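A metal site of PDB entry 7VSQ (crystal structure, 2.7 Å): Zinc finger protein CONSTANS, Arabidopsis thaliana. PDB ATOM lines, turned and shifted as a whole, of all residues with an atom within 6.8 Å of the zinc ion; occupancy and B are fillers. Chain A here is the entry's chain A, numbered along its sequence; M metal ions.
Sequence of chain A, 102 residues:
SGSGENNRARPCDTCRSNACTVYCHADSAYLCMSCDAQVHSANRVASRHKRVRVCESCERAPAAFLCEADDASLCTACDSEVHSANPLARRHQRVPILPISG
The backbone NH of Cys 55 sits at hydrogen-bond distance from the backbone carbonyl oxygen of Ala 61 (3.0 Å). The side-chain sulfur of Cys 55 sits close to the backbone NH of Ser 57 (3.2 Å).
Four residues have an atom within 4 Å of the zinc ion: Cys 55, Cys 58, Cys 75 and Cys 78.
The zinc ion is bound by the side-chain sulfur (SG) of Cys 75 (2.1 Å), the side-chain sulfur (SG) of Cys 55 (2.4 Å), the side-chain sulfur (SG) of Cys 58 (2.4 Å) and the side-chain sulfur (SG) of Cys 78 (2.4 Å).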
ATOM      1  N   CYS A  55      26.905 -20.264 -17.234  1.00  0.00           N
ATOM      2  CA  CYS A  55      27.123 -18.836 -17.085  1.00  0.00           C
ATOM      3  C   CYS A  55      27.276 -18.517 -15.608  1.00  0.00           C
ATOM      4  O   CYS A  55      26.489 -18.998 -14.789  1.00  0.00           O
ATOM      5  CB  CYS A  55      25.956 -18.061 -17.679  1.00  0.00           C
ATOM      6  SG  CYS A  55      26.037 -16.308 -17.414  1.00  0.00           S
ATOM      7  N   GLU A  56      28.241 -17.677 -15.279  1.00  0.00           N
ATOM      8  CA  GLU A  56      28.481 -17.338 -13.896  1.00  0.00           C
ATOM      9  C   GLU A  56      27.575 -16.221 -13.437  1.00  0.00           C
ATOM     10  O   GLU A  56      27.585 -15.870 -12.282  1.00  0.00           O
ATOM     11  CB  GLU A  56      29.930 -16.973 -13.651  1.00  0.00           C
ATOM     12  CG  GLU A  56      30.871 -18.141 -13.736  1.00  0.00           C
ATOM     13  CD  GLU A  56      32.316 -17.728 -13.820  1.00  0.00           C
ATOM     14  OE1 GLU A  56      32.785 -17.402 -14.915  1.00  0.00           O
ATOM     15  OE2 GLU A  56      32.985 -17.730 -12.784  1.00  0.00           O
ATOM     16  N   SER A  57      26.756 -15.710 -14.338  1.00  0.00           N
ATOM     17  CA  SER A  57      25.806 -14.697 -13.964  1.00  0.00           C
ATOM     18  C   SER A  57      24.406 -15.262 -13.816  1.00  0.00           C
ATOM     19  O   SER A  57      23.911 -15.344 -12.710  1.00  0.00           O
ATOM     20  CB  SER A  57      25.802 -13.602 -15.002  1.00  0.00           C
ATOM     21  OG  SER A  57      24.763 -12.691 -14.785  1.00  0.00           O
ATOM     22  N   CYS A  58      23.765 -15.644 -14.901  1.00  0.00           N
ATOM     23  CA  CYS A  58      22.457 -16.268 -14.800  1.00  0.00           C
ATOM     24  C   CYS A  58      22.381 -17.644 -14.199  1.00  0.00           C
ATOM     25  O   CYS A  58      21.410 -17.976 -13.580  1.00  0.00           O
ATOM     26  CB  CYS A  58      21.567 -16.146 -16.040  1.00  0.00           C
ATOM     27  SG  CYS A  58      22.116 -16.859 -17.580  1.00  0.00           S
ATOM     28  N   GLU A  59      23.367 -18.475 -14.453  1.00  0.00           N
ATOM     29  CA  GLU A  59      23.476 -19.747 -13.769  1.00  0.00           C
ATOM     30  C   GLU A  59      22.473 -20.751 -14.288  1.00  0.00           C
ATOM     31  O   GLU A  59      22.265 -21.774 -13.686  1.00  0.00           O
ATOM     32  CB  GLU A  59      23.247 -19.559 -12.275  1.00  0.00           C
ATOM     33  CG  GLU A  59      24.506 -19.314 -11.466  1.00  0.00           C
ATOM     34  CD  GLU A  59      24.234 -19.105  -9.987  1.00  0.00           C
ATOM     35  OE1 GLU A  59      23.530 -18.137  -9.619  1.00  0.00           O
ATOM     36  OE2 GLU A  59      24.750 -19.898  -9.176  1.00  0.00           O
ATOM     37  N   ARG A  60      21.819 -20.419 -15.381  1.00  0.00           N
ATOM     38  CA  ARG A  60      20.791 -21.233 -15.967  1.00  0.00           C
ATOM     39  C   ARG A  60      21.083 -21.592 -17.410  1.00  0.00           C
ATOM     40  O   ARG A  60      20.181 -21.902 -18.165  1.00  0.00           O
ATOM     41  CB  ARG A  60      19.489 -20.457 -15.919  1.00  0.00           C
ATOM     42  CG  ARG A  60      18.286 -21.187 -16.484  1.00  0.00           C
ATOM     43  CD  ARG A  60      17.007 -20.390 -16.338  1.00  0.00           C
ATOM     44  NE  ARG A  60      17.009 -19.151 -17.122  1.00  0.00           N
ATOM     45  CZ  ARG A  60      16.710 -19.086 -18.408  1.00  0.00           C
ATOM     46  NH1 ARG A  60      16.335 -20.166 -19.073  1.00  0.00           N
ATOM     47  NH2 ARG A  60      16.766 -17.924 -19.016  1.00  0.00           N
ATOM     48  N   ALA A  61      22.323 -21.461 -17.835  1.00  0.00           N
ATOM     49  CA  ALA A  61      22.625 -21.441 -19.249  1.00  0.00           C
ATOM     50  C   ALA A  61      24.052 -21.831 -19.531  1.00  0.00           C
ATOM     51  O   ALA A  61      24.815 -21.994 -18.624  1.00  0.00           O
ATOM     52  CB  ALA A  61      22.367 -20.075 -19.803  1.00  0.00           C
ATOM     53  N   PRO A  62      24.394 -22.002 -20.785  1.00  0.00           N
ATOM     54  CA  PRO A  62      25.807 -22.222 -21.127  1.00  0.00           C
ATOM     55  C   PRO A  62      26.474 -20.921 -21.593  1.00  0.00           C
ATOM     56  O   PRO A  62      25.808 -20.056 -22.166  1.00  0.00           O
ATOM     57  CB  PRO A  62      25.733 -23.245 -22.257  1.00  0.00           C
ATOM     58  CG  PRO A  62      24.408 -22.982 -22.904  1.00  0.00           C
ATOM     59  CD  PRO A  62      23.487 -22.592 -21.788  1.00  0.00           C
ATOM     60  N   ALA A  63      27.765 -20.800 -21.329  1.00  0.00           N
ATOM     61  CA  ALA A  63      28.536 -19.595 -21.654  1.00  0.00           C
ATOM     62  C   ALA A  63      29.033 -19.559 -23.106  1.00  0.00           C
ATOM     63  O   ALA A  63      29.606 -20.525 -23.603  1.00  0.00           O
ATOM     64  CB  ALA A  63      29.710 -19.455 -20.710  1.00  0.00           C
ATOM     65  N   SER A  73      32.531 -16.084 -17.334  1.00  0.00           N
ATOM     66  CA  SER A  73      31.998 -16.684 -18.564  1.00  0.00           C
ATOM     67  C   SER A  73      30.463 -16.623 -18.605  1.00  0.00           C
ATOM     68  O   SER A  73      29.786 -17.105 -17.699  1.00  0.00           O
ATOM     69  CB  SER A  73      32.485 -18.120 -18.719  1.00  0.00           C
ATOM     70  OG  SER A  73      33.907 -18.185 -18.660  1.00  0.00           O
ATOM     71  N   LEU A  74      29.931 -16.009 -19.658  1.00  0.00           N
ATOM     72  CA  LEU A  74      28.517 -15.641 -19.754  1.00  0.00           C
ATOM     73  C   LEU A  74      27.849 -16.051 -21.070  1.00  0.00           C
ATOM     74  O   LEU A  74      28.531 -16.264 -22.086  1.00  0.00           O
ATOM     75  CB  LEU A  74      28.376 -14.133 -19.597  1.00  0.00           C
ATOM     76  CG  LEU A  74      29.276 -13.489 -18.562  1.00  0.00           C
ATOM     77  CD1 LEU A  74      29.381 -11.987 -18.797  1.00  0.00           C
ATOM     78  CD2 LEU A  74      28.777 -13.783 -17.162  1.00  0.00           C
ATOM     79  N   CYS A  75      26.524 -16.170 -21.024  1.00  0.00           N
ATOM     80  CA  CYS A  75      25.704 -16.475 -22.190  1.00  0.00           C
ATOM     81  C   CYS A  75      25.793 -15.316 -23.138  1.00  0.00           C
ATOM     82  O   CYS A  75      26.182 -14.241 -22.728  1.00  0.00           O
ATOM     83  CB  CYS A  75      24.237 -16.672 -21.836  1.00  0.00           C
ATOM     84  SG  CYS A  75      23.900 -17.072 -20.139  1.00  0.00           S
ATOM     85  N   THR A  76      25.359 -15.498 -24.377  1.00  0.00           N
ATOM     86  CA  THR A  76      25.268 -14.408 -25.338  1.00  0.00           C
ATOM     87  C   THR A  76      24.431 -13.276 -24.754  1.00  0.00           C
ATOM     88  O   THR A  76      24.864 -12.125 -24.705  1.00  0.00           O
ATOM     89  CB  THR A  76      24.662 -14.876 -26.679  1.00  0.00           C
ATOM     90  OG1 THR A  76      25.688 -15.394 -27.535  1.00  0.00           O
ATOM     91  CG2 THR A  76      23.976 -13.719 -27.398  1.00  0.00           C
ATOM     92  N   ALA A  77      23.229 -13.623 -24.298  1.00  0.00           N
ATOM     93  CA  ALA A  77      22.303 -12.647 -23.741  1.00  0.00           C
ATOM     94  C   ALA A  77      22.900 -11.916 -22.544  1.00  0.00           C
ATOM     95  O   ALA A  77      22.917 -10.689 -22.499  1.00  0.00           O
ATOM     96  CB  ALA A  77      21.007 -13.324 -23.337  1.00  0.00           C
ATOM     97  N   CYS A  78      23.385 -12.680 -21.568  1.00  0.00           N
ATOM     98  CA  CYS A  78      23.929 -12.095 -20.355  1.00  0.00           C
ATOM     99  C   CYS A  78      25.277 -11.416 -20.598  1.00  0.00           C
ATOM    100  O   CYS A  78      25.609 -10.441 -19.922  1.00  0.00           O
ATOM    101  CB  CYS A  78      24.041 -13.154 -19.276  1.00  0.00           C
ATOM    102  SG  CYS A  78      22.440 -13.878 -18.899  1.00  0.00           S
ATOM    103  N   ASP A  79      26.027 -11.914 -21.569  1.00  0.00           N
ATOM    104  CA  ASP A  79      27.265 -11.264 -21.973  1.00  0.00           C
ATOM    105  C   ASP A  79      26.961  -9.880 -22.505  1.00  0.00           C
ATOM    106  O   ASP A  79      27.627  -8.902 -22.157  1.00  0.00           O
ATOM    107  CB  ASP A  79      28.000 -12.095 -23.029  1.00  0.00           C
ATOM    108  CG  ASP A  79      29.202 -11.400 -23.607  1.00  0.00           C
ATOM    109  OD1 ASP A  79      29.046 -10.662 -24.602  1.00  0.00           O
ATOM    110  OD2 ASP A  79      30.295 -11.600 -23.044  1.00  0.00           O
HETATM  111 ZN    ZN M   1      23.996 -15.702 -18.511  1.00  0.00          ZN
